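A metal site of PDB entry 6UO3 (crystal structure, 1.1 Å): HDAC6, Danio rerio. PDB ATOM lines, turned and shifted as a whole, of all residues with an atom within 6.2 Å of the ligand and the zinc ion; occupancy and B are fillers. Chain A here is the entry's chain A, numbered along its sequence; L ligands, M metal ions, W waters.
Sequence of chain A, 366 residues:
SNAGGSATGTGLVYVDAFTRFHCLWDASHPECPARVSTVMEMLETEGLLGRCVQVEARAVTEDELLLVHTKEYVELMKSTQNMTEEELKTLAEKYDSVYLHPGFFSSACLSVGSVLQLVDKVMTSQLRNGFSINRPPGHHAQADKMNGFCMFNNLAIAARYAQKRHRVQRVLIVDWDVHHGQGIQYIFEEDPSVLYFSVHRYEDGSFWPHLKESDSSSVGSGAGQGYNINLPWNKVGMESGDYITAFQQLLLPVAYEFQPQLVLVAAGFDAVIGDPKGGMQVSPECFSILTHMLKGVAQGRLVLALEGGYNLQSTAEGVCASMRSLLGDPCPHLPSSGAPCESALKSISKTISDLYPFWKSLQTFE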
ATOM      1  N   ASP A  26     -24.090   8.402 -27.876  1.00  0.00           N
ATOM      2  CA  ASP A  26     -22.681   8.431 -28.244  1.00  0.00           C
ATOM      3  C   ASP A  26     -21.955   7.447 -27.330  1.00  0.00           C
ATOM      4  O   ASP A  26     -21.593   7.805 -26.213  1.00  0.00           O
ATOM      5  CB  ASP A  26     -22.101   9.836 -28.122  1.00  0.00           C
ATOM      6  CG  ASP A  26     -20.613   9.888 -28.428  1.00  0.00           C
ATOM      7  OD1 ASP A  26     -20.046   8.854 -28.840  1.00  0.00           O
ATOM      8  OD2 ASP A  26     -20.014  10.967 -28.254  1.00  0.00           O
ATOM      9  N   SER A  28     -19.058   6.464 -27.387  1.00  0.00           N
ATOM     10  CA  SER A  28     -17.684   6.847 -27.107  1.00  0.00           C
ATOM     11  C   SER A  28     -17.577   8.154 -26.322  1.00  0.00           C
ATOM     12  O   SER A  28     -16.490   8.721 -26.223  1.00  0.00           O
ATOM     13  CB  SER A  28     -16.874   6.955 -28.406  1.00  0.00           C
ATOM     14  OG  SER A  28     -16.838   5.708 -29.068  1.00  0.00           O
ATOM     15  N   HIS A  29     -18.683   8.632 -25.751  1.00  0.00           N
ATOM     16  CA  HIS A  29     -18.625   9.888 -25.014  1.00  0.00           C
ATOM     17  C   HIS A  29     -17.611   9.760 -23.889  1.00  0.00           C
ATOM     18  O   HIS A  29     -17.606   8.753 -23.170  1.00  0.00           O
ATOM     19  CB  HIS A  29     -19.987  10.238 -24.424  1.00  0.00           C
ATOM     20  CG  HIS A  29     -20.091  11.665 -23.993  1.00  0.00           C
ATOM     21  ND1 HIS A  29     -19.480  12.151 -22.854  1.00  0.00           N
ATOM     22  CD2 HIS A  29     -20.713  12.728 -24.565  1.00  0.00           C
ATOM     23  CE1 HIS A  29     -19.725  13.452 -22.745  1.00  0.00           C
ATOM     24  NE2 HIS A  29     -20.472  13.822 -23.772  1.00  0.00           N
ATOM     25  N   PRO A  30     -16.736  10.753 -23.684  1.00  0.00           N
ATOM     26  CA  PRO A  30     -15.688  10.619 -22.671  1.00  0.00           C
ATOM     27  C   PRO A  30     -16.187  10.693 -21.237  1.00  0.00           C
ATOM     28  O   PRO A  30     -15.505  10.169 -20.340  1.00  0.00           O
ATOM     29  CB  PRO A  30     -14.720  11.768 -22.984  1.00  0.00           C
ATOM     30  CG  PRO A  30     -15.605  12.807 -23.618  1.00  0.00           C
ATOM     31  CD  PRO A  30     -16.609  12.012 -24.446  1.00  0.00           C
ATOM     32  N   SER A  97     -22.198  21.426 -25.181  1.00  0.00           N
ATOM     33  CA  SER A  97     -21.394  20.293 -24.754  1.00  0.00           C
ATOM     34  C   SER A  97     -21.980  19.554 -23.537  1.00  0.00           C
ATOM     35  O   SER A  97     -21.301  19.358 -22.528  1.00  0.00           O
ATOM     36  CB  SER A  97     -19.942  20.718 -24.522  1.00  0.00           C
ATOM     37  OG  SER A  97     -19.136  19.609 -24.196  1.00  0.00           O
ATOM     38  N   VAL A  98     -23.227  19.115 -23.671  1.00  0.00           N
ATOM     39  CA  VAL A  98     -23.836  18.269 -22.644  1.00  0.00           C
ATOM     40  C   VAL A  98     -24.688  17.191 -23.283  1.00  0.00           C
ATOM     41  O   VAL A  98     -25.197  17.349 -24.401  1.00  0.00           O
ATOM     42  CB  VAL A  98     -24.717  19.050 -21.642  1.00  0.00           C
ATOM     43  CG1 VAL A  98     -23.912  20.155 -20.996  1.00  0.00           C
ATOM     44  CG2 VAL A  98     -25.940  19.614 -22.320  1.00  0.00           C
ATOM     45  N   PRO A 137     -19.713  16.180 -13.132  1.00  0.00           N
ATOM     46  CA  PRO A 137     -18.909  17.318 -12.690  1.00  0.00           C
ATOM     47  C   PRO A 137     -19.770  18.577 -12.591  1.00  0.00           C
ATOM     48  O   PRO A 137     -20.949  18.581 -12.959  1.00  0.00           O
ATOM     49  CB  PRO A 137     -17.869  17.439 -13.806  1.00  0.00           C
ATOM     50  CG  PRO A 137     -18.596  16.961 -15.031  1.00  0.00           C
ATOM     51  CD  PRO A 137     -19.446  15.811 -14.538  1.00  0.00           C
ATOM     52  N   HIS A 139     -18.086  22.344 -12.527  1.00  0.00           N
ATOM     53  CA  HIS A 139     -17.526  23.707 -12.559  1.00  0.00           C
ATOM     54  C   HIS A 139     -17.984  24.566 -13.739  1.00  0.00           C
ATOM     55  O   HIS A 139     -17.809  25.792 -13.685  1.00  0.00           O
ATOM     56  CB  HIS A 139     -16.005  23.740 -12.373  1.00  0.00           C
ATOM     57  CG  HIS A 139     -15.209  23.123 -13.490  1.00  0.00           C
ATOM     58  ND1 HIS A 139     -13.921  23.543 -13.774  1.00  0.00           N
ATOM     59  CD2 HIS A 139     -15.485  22.122 -14.344  1.00  0.00           C
ATOM     60  CE1 HIS A 139     -13.446  22.823 -14.768  1.00  0.00           C
ATOM     61  NE2 HIS A 139     -14.368  21.950 -15.144  1.00  0.00           N
ATOM     62  N   HIS A 140     -18.542  23.968 -14.789  1.00  0.00           N
ATOM     63  CA  HIS A 140     -19.072  24.744 -15.913  1.00  0.00           C
ATOM     64  C   HIS A 140     -20.537  25.108 -15.742  1.00  0.00           C
ATOM     65  O   HIS A 140     -21.032  25.973 -16.485  1.00  0.00           O
ATOM     66  CB  HIS A 140     -18.938  23.959 -17.219  1.00  0.00           C
ATOM     67  CG  HIS A 140     -17.533  23.634 -17.583  1.00  0.00           C
ATOM     68  ND1 HIS A 140     -16.573  24.602 -17.789  1.00  0.00           N
ATOM     69  CD2 HIS A 140     -16.918  22.443 -17.804  1.00  0.00           C
ATOM     70  CE1 HIS A 140     -15.426  24.029 -18.101  1.00  0.00           C
ATOM     71  NE2 HIS A 140     -15.621  22.713 -18.131  1.00  0.00           N
ATOM     72  N   GLY A 148     -20.885  22.002 -20.560  1.00  0.00           N
ATOM     73  CA  GLY A 148     -19.639  21.272 -20.358  1.00  0.00           C
ATOM     74  C   GLY A 148     -19.726  20.049 -19.473  1.00  0.00           C
ATOM     75  O   GLY A 148     -18.898  19.866 -18.565  1.00  0.00           O
ATOM     76  N   PHE A 149     -20.705  19.191 -19.743  1.00  0.00           N
ATOM     77  CA  PHE A 149     -20.946  17.938 -19.030  1.00  0.00           C
ATOM     78  C   PHE A 149     -21.519  18.140 -17.633  1.00  0.00           C
ATOM     79  O   PHE A 149     -21.665  17.156 -16.894  1.00  0.00           O
ATOM     80  CB  PHE A 149     -19.712  17.019 -18.939  1.00  0.00           C
ATOM     81  CG  PHE A 149     -19.002  16.769 -20.260  1.00  0.00           C
ATOM     82  CD1 PHE A 149     -17.680  16.352 -20.259  1.00  0.00           C
ATOM     83  CD2 PHE A 149     -19.657  16.907 -21.472  1.00  0.00           C
ATOM     84  CE1 PHE A 149     -17.007  16.092 -21.434  1.00  0.00           C
ATOM     85  CE2 PHE A 149     -18.978  16.650 -22.664  1.00  0.00           C
ATOM     86  CZ  PHE A 149     -17.654  16.248 -22.635  1.00  0.00           C
ATOM     87  N   CYS A 150     -21.890  19.370 -17.263  1.00  0.00           N
ATOM     88  CA  CYS A 150     -22.305  19.724 -15.903  1.00  0.00           C
ATOM     89  C   CYS A 150     -23.752  20.187 -15.884  1.00  0.00           C
ATOM     90  O   CYS A 150     -24.194  20.945 -16.753  1.00  0.00           O
ATOM     91  CB  CYS A 150     -21.441  20.874 -15.359  1.00  0.00           C
ATOM     92  SG  CYS A 150     -19.668  20.599 -15.353  1.00  0.00           S
ATOM     93  N   ASP A 177      -8.497  21.569 -12.864  1.00  0.00           N
ATOM     94  CA  ASP A 177      -8.953  20.957 -14.104  1.00  0.00           C
ATOM     95  C   ASP A 177      -8.358  21.730 -15.282  1.00  0.00           C
ATOM     96  O   ASP A 177      -8.090  22.929 -15.195  1.00  0.00           O
ATOM     97  CB  ASP A 177     -10.480  21.030 -14.124  1.00  0.00           C
ATOM     98  CG  ASP A 177     -11.102  20.268 -15.262  1.00  0.00           C
ATOM     99  OD1 ASP A 177     -11.094  20.764 -16.417  1.00  0.00           O
ATOM    100  OD2 ASP A 177     -11.638  19.160 -15.002  1.00  0.00           O
ATOM    101  N   VAL A 178      -8.128  21.023 -16.392  1.00  0.00           N
ATOM    102  CA  VAL A 178      -7.497  21.659 -17.547  1.00  0.00           C
ATOM    103  C   VAL A 178      -8.398  22.688 -18.218  1.00  0.00           C
ATOM    104  O   VAL A 178      -7.905  23.514 -19.018  1.00  0.00           O
ATOM    105  CB  VAL A 178      -7.007  20.590 -18.548  1.00  0.00           C
ATOM    106  CG1 VAL A 178      -8.150  20.151 -19.477  1.00  0.00           C
ATOM    107  CG2 VAL A 178      -5.811  21.096 -19.349  1.00  0.00           C
ATOM    108  N   HIS A 179      -9.688  22.664 -17.946  1.00  0.00           N
ATOM    109  CA  HIS A 179     -10.629  23.626 -18.510  1.00  0.00           C
ATOM    110  C   HIS A 179     -10.918  24.739 -17.516  1.00  0.00           C
ATOM    111  O   HIS A 179     -10.854  24.546 -16.294  1.00  0.00           O
ATOM    112  CB  HIS A 179     -11.952  22.939 -18.840  1.00  0.00           C
ATOM    113  CG  HIS A 179     -11.832  21.861 -19.874  1.00  0.00           C
ATOM    114  ND1 HIS A 179     -11.619  20.533 -19.543  1.00  0.00           N
ATOM    115  CD2 HIS A 179     -11.892  21.915 -21.219  1.00  0.00           C
ATOM    116  CE1 HIS A 179     -11.554  19.829 -20.664  1.00  0.00           C
ATOM    117  NE2 HIS A 179     -11.706  20.640 -21.687  1.00  0.00           N
ATOM    118  N   TRP A 208     -11.505  24.920 -25.964  1.00  0.00           N
ATOM    119  CA  TRP A 208     -12.826  25.066 -25.390  1.00  0.00           C
ATOM    120  C   TRP A 208     -12.708  25.480 -23.928  1.00  0.00           C
ATOM    121  O   TRP A 208     -11.850  24.954 -23.201  1.00  0.00           O
ATOM    122  CB  TRP A 208     -13.548  23.717 -25.514  1.00  0.00           C
ATOM    123  CG  TRP A 208     -15.005  23.794 -25.222  1.00  0.00           C
ATOM    124  CD1 TRP A 208     -16.013  23.972 -26.117  1.00  0.00           C
ATOM    125  CD2 TRP A 208     -15.618  23.716 -23.933  1.00  0.00           C
ATOM    126  NE1 TRP A 208     -17.219  24.015 -25.463  1.00  0.00           N
ATOM    127  CE2 TRP A 208     -16.994  23.868 -24.119  1.00  0.00           C
ATOM    128  CE3 TRP A 208     -15.120  23.548 -22.630  1.00  0.00           C
ATOM    129  CZ2 TRP A 208     -17.900  23.849 -23.048  1.00  0.00           C
ATOM    130  CZ3 TRP A 208     -16.012  23.538 -21.584  1.00  0.00           C
ATOM    131  CH2 TRP A 208     -17.386  23.688 -21.794  1.00  0.00           C
ATOM    132  N   HIS A 210     -13.365  28.605 -25.284  1.00  0.00           N
ATOM    133  CA  HIS A 210     -13.137  29.693 -26.245  1.00  0.00           C
ATOM    134  C   HIS A 210     -13.628  31.052 -25.768  1.00  0.00           C
ATOM    135  O   HIS A 210     -14.129  31.844 -26.579  1.00  0.00           O
ATOM    136  CB  HIS A 210     -13.815  29.410 -27.592  1.00  0.00           C
ATOM    137  CG  HIS A 210     -13.655  27.999 -28.058  1.00  0.00           C
ATOM    138  ND1 HIS A 210     -12.446  27.493 -28.475  1.00  0.00           N
ATOM    139  CD2 HIS A 210     -14.548  26.992 -28.185  1.00  0.00           C
ATOM    140  CE1 HIS A 210     -12.603  26.233 -28.853  1.00  0.00           C
ATOM    141  NE2 HIS A 210     -13.870  25.900 -28.678  1.00  0.00           N
ATOM    142  N   GLY A 268     -10.184  18.234 -11.209  1.00  0.00           N
ATOM    143  CA  GLY A 268     -10.137  17.506 -12.457  1.00  0.00           C
ATOM    144  C   GLY A 268      -8.744  16.969 -12.707  1.00  0.00           C
ATOM    145  O   GLY A 268      -7.759  17.484 -12.170  1.00  0.00           O
ATOM    146  N   ASP A 270      -7.791  16.070 -16.072  1.00  0.00           N
ATOM    147  CA  ASP A 270      -7.555  16.127 -17.495  1.00  0.00           C
ATOM    148  C   ASP A 270      -6.269  16.854 -17.866  1.00  0.00           C
ATOM    149  O   ASP A 270      -5.921  16.876 -19.049  1.00  0.00           O
ATOM    150  CB  ASP A 270      -8.772  16.640 -18.284  1.00  0.00           C
ATOM    151  CG  ASP A 270      -9.519  17.778 -17.586  1.00  0.00           C
ATOM    152  OD1 ASP A 270      -8.972  18.405 -16.645  1.00  0.00           O
ATOM    153  OD2 ASP A 270     -10.672  18.023 -18.015  1.00  0.00           O
ATOM    154  N   LYS A 277      -8.086  14.713 -23.909  1.00  0.00           N
ATOM    155  CA  LYS A 277      -8.553  16.060 -24.206  1.00  0.00           C
ATOM    156  C   LYS A 277      -7.580  17.155 -23.782  1.00  0.00           C
ATOM    157  O   LYS A 277      -7.461  18.171 -24.465  1.00  0.00           O
ATOM    158  CB  LYS A 277      -9.891  16.315 -23.499  1.00  0.00           C
ATOM    159  CG  LYS A 277     -11.032  15.488 -24.058  1.00  0.00           C
ATOM    160  CD  LYS A 277     -11.238  15.802 -25.532  1.00  0.00           C
ATOM    161  CE  LYS A 277     -12.451  15.100 -26.091  1.00  0.00           C
ATOM    162  NZ  LYS A 277     -12.593  15.369 -27.544  1.00  0.00           N
ATOM    163  N   GLU A 307     -13.858  16.732 -10.928  1.00  0.00           N
ATOM    164  CA  GLU A 307     -14.399  17.415 -12.093  1.00  0.00           C
ATOM    165  C   GLU A 307     -14.123  16.540 -13.316  1.00  0.00           C
ATOM    166  O   GLU A 307     -14.677  15.429 -13.406  1.00  0.00           O
ATOM    167  CB  GLU A 307     -13.832  18.848 -12.204  1.00  0.00           C
ATOM    168  CG  GLU A 307     -14.175  19.754 -11.005  1.00  0.00           C
ATOM    169  CD  GLU A 307     -15.588  20.319 -11.010  1.00  0.00           C
ATOM    170  OE1 GLU A 307     -15.941  21.023 -10.027  1.00  0.00           O
ATOM    171  OE2 GLU A 307     -16.360  20.070 -11.972  1.00  0.00           O
ATOM    172  N   GLY A 308     -13.266  16.984 -14.244  1.00  0.00           N
ATOM    173  CA  GLY A 308     -12.952  16.225 -15.426  1.00  0.00           C
ATOM    174  C   GLY A 308     -11.790  15.258 -15.236  1.00  0.00           C
ATOM    175  O   GLY A 308     -11.342  14.969 -14.127  1.00  0.00           O
ATOM    176  N   GLY A 309     -11.289  14.767 -16.373  1.00  0.00           N
ATOM    177  CA  GLY A 309     -10.284  13.714 -16.396  1.00  0.00           C
ATOM    178  C   GLY A 309     -10.854  12.490 -17.072  1.00  0.00           C
ATOM    179  O   GLY A 309     -11.795  11.871 -16.552  1.00  0.00           O
ATOM    180  N   TYR A 310     -10.312  12.135 -18.231  1.00  0.00           N
ATOM    181  CA  TYR A 310     -10.964  11.201 -19.146  1.00  0.00           C
ATOM    182  C   TYR A 310     -10.122   9.995 -19.539  1.00  0.00           C
ATOM    183  O   TYR A 310     -10.658   9.082 -20.173  1.00  0.00           O
ATOM    184  CB  TYR A 310     -11.485  11.956 -20.386  1.00  0.00           C
ATOM    185  CG  TYR A 310     -12.380  13.049 -19.928  1.00  0.00           C
ATOM    186  CD1 TYR A 310     -13.654  12.764 -19.466  1.00  0.00           C
ATOM    187  CD2 TYR A 310     -11.921  14.355 -19.817  1.00  0.00           C
ATOM    188  CE1 TYR A 310     -14.471  13.761 -18.977  1.00  0.00           C
ATOM    189  CE2 TYR A 310     -12.725  15.354 -19.324  1.00  0.00           C
ATOM    190  CZ  TYR A 310     -13.995  15.056 -18.906  1.00  0.00           C
ATOM    191  OH  TYR A 310     -14.799  16.046 -18.407  1.00  0.00           O
HETATM  192  C1  LIG L   1     -15.903  19.110 -27.928  1.00  0.00           C
HETATM  193  C2  LIG L   1     -17.107  17.177 -26.724  1.00  0.00           C
HETATM  194  C3  LIG L   1     -18.864  15.524 -26.525  1.00  0.00           C
HETATM  195  C4  LIG L   1     -16.661  14.789 -27.030  1.00  0.00           C
HETATM  196  C5  LIG L   1     -14.799  18.303 -22.522  1.00  0.00           C
HETATM  197  C6  LIG L   1     -14.324  18.291 -21.247  1.00  0.00           C
HETATM  198  C7  LIG L   1     -14.229  19.137 -18.940  1.00  0.00           C
HETATM  199  C8  LIG L   1     -14.829  19.141 -20.288  1.00  0.00           C
HETATM  200  C9  LIG L   1     -15.828  20.032 -20.735  1.00  0.00           C
HETATM  201  C10 LIG L   1     -16.305  20.037 -22.042  1.00  0.00           C
HETATM  202  C11 LIG L   1     -15.806  19.159 -22.970  1.00  0.00           C
HETATM  203  C12 LIG L   1     -15.763  18.738 -25.459  1.00  0.00           C
HETATM  204  C13 LIG L   1     -16.639  18.639 -26.644  1.00  0.00           C
HETATM  205  C14 LIG L   1     -15.351  20.538 -27.806  1.00  0.00           C
HETATM  206  C15 LIG L   1     -16.781  19.056 -29.175  1.00  0.00           C
HETATM  207  C16 LIG L   1     -18.427  16.837 -26.482  1.00  0.00           C
HETATM  208  C17 LIG L   1     -17.987  14.481 -26.792  1.00  0.00           C
HETATM  209  C18 LIG L   1     -16.227  16.122 -26.973  1.00  0.00           C
HETATM  210  N1  LIG L   1     -16.151  19.049 -24.237  1.00  0.00           N
HETATM  211  N2  LIG L   1     -14.400  20.271 -18.113  1.00  0.00           N
HETATM  212  O1  LIG L   1     -13.497  18.269 -18.530  1.00  0.00           O
HETATM  213  O2  LIG L   1     -14.566  18.479 -25.564  1.00  0.00           O
HETATM  214  O3  LIG L   1     -13.835  20.312 -16.886  1.00  0.00           O
HETATM  215 ZN    ZN M   1     -11.962  19.554 -17.695  1.00  0.00          ZN
HETATM  216  O   HOH W   1     -21.671  17.679 -27.139  1.00  0.00           O
HETATM  217  O   HOH W   2     -12.773  17.956 -27.600  1.00  0.00           O
HETATM  218  O   HOH W   3     -12.058  19.574 -24.258  1.00  0.00           O
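An oxygen (O3) of the ligand lies close to a ring nitrogen (NE2) of His 139 (2.4 Å). The side-chain hydroxyl of Tyr 310 sits close to an oxygen (O1) of the ligand, at 2.6 Å. N2 of the ligand lies close to NE2 of His 140 (2.7 Å). A nitrogen (N1) of the ligand lies within hydrogen-bond range of the side-chain hydroxyl (OG) of Ser 97 (3.0 Å).
The backbone NH of Gly 308 is in hydrogen-bond range of the side-chain carboxylate of Asp 177 (2.8 Å). A ring nitrogen (NE2) of His 140 sits at hydrogen-bond distance from a ring nitrogen (NE2) of His 139, at 3.3 Å. The side-chain carboxylate (OE2) of Glu 307 sits at hydrogen-bond distance from the backbone NH (N) of His 139, 2.9 Å away. The side-chain sulfur of Cys 150 lies within hydrogen-bond range of the backbone NH of His 139, at 3.7 Å. N of His 140 sits at hydrogen-bond distance from SG of Cys 150 (3.6 Å). The backbone carbonyl oxygen (O) of Ser 97 lies within hydrogen-bond range of the backbone NH (N) of Phe 149. The side-chain carboxylate (OD1) of Asp 26 is in hydrogen-bond range of the backbone NH (N) of His 29. The side-chain sulfur of Cys 150 is in hydrogen-bond range of the backbone carbonyl oxygen of Gly 148.
His 29 touches the ligand. CD of Pro 30 touches C17 of the ligand (3.7 Å). Gly 148 touches the ligand. Phe 149 touches the ligand (CE1 to C5, 3.3 Å). CZ3 of Trp 208 touches C10 of the ligand, at 3.5 Å. Lys 277 touches the ligand. Gly 308 touches the ligand. Hydrophobic or aromatic side chains that line the ligand: His 29, Pro 30, His 139, His 140, Phe 149, His 179, Trp 208 and Tyr 310. 14 residues have an atom within 4 Å of the ligand: His 29, Pro 30, Ser 97, His 139, His 140, Gly 148, Phe 149, Asp 177, His 179, Trp 208, Asp 270, Lys 277, Gly 308 and Tyr 310. The nearest printed residue that does not touch the ligand is Asp 26 (4.3 Å).
The nearest printed residue that does not touch the zinc ion is Gly 308 (4.1 Å).
The zinc ion is bound by OD1 of Asp 177, at 2.0 Å. OD2 of Asp 270 binds the zinc ion, at 2.0 Å. A ring nitrogen (ND1) of His 179 binds the zinc ion. O1 of the ligand binds the zinc ion (2.2 Å). O3 of the ligand binds the zinc ion. The zinc ion has five donor atoms within binding distance. Slightly farther from the zinc ion lies OD2 of Asp 177 (2.7 Å).
Water W2 lies within hydrogen-bond range of the side-chain amino group (NZ) of Lys 277 (2.6 Å) and an oxygen (O2) of the ligand (2.8 Å). Water W3 bridges NE2 of His 179 (2.8 Å) and O2 of the ligand (3.0 Å).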
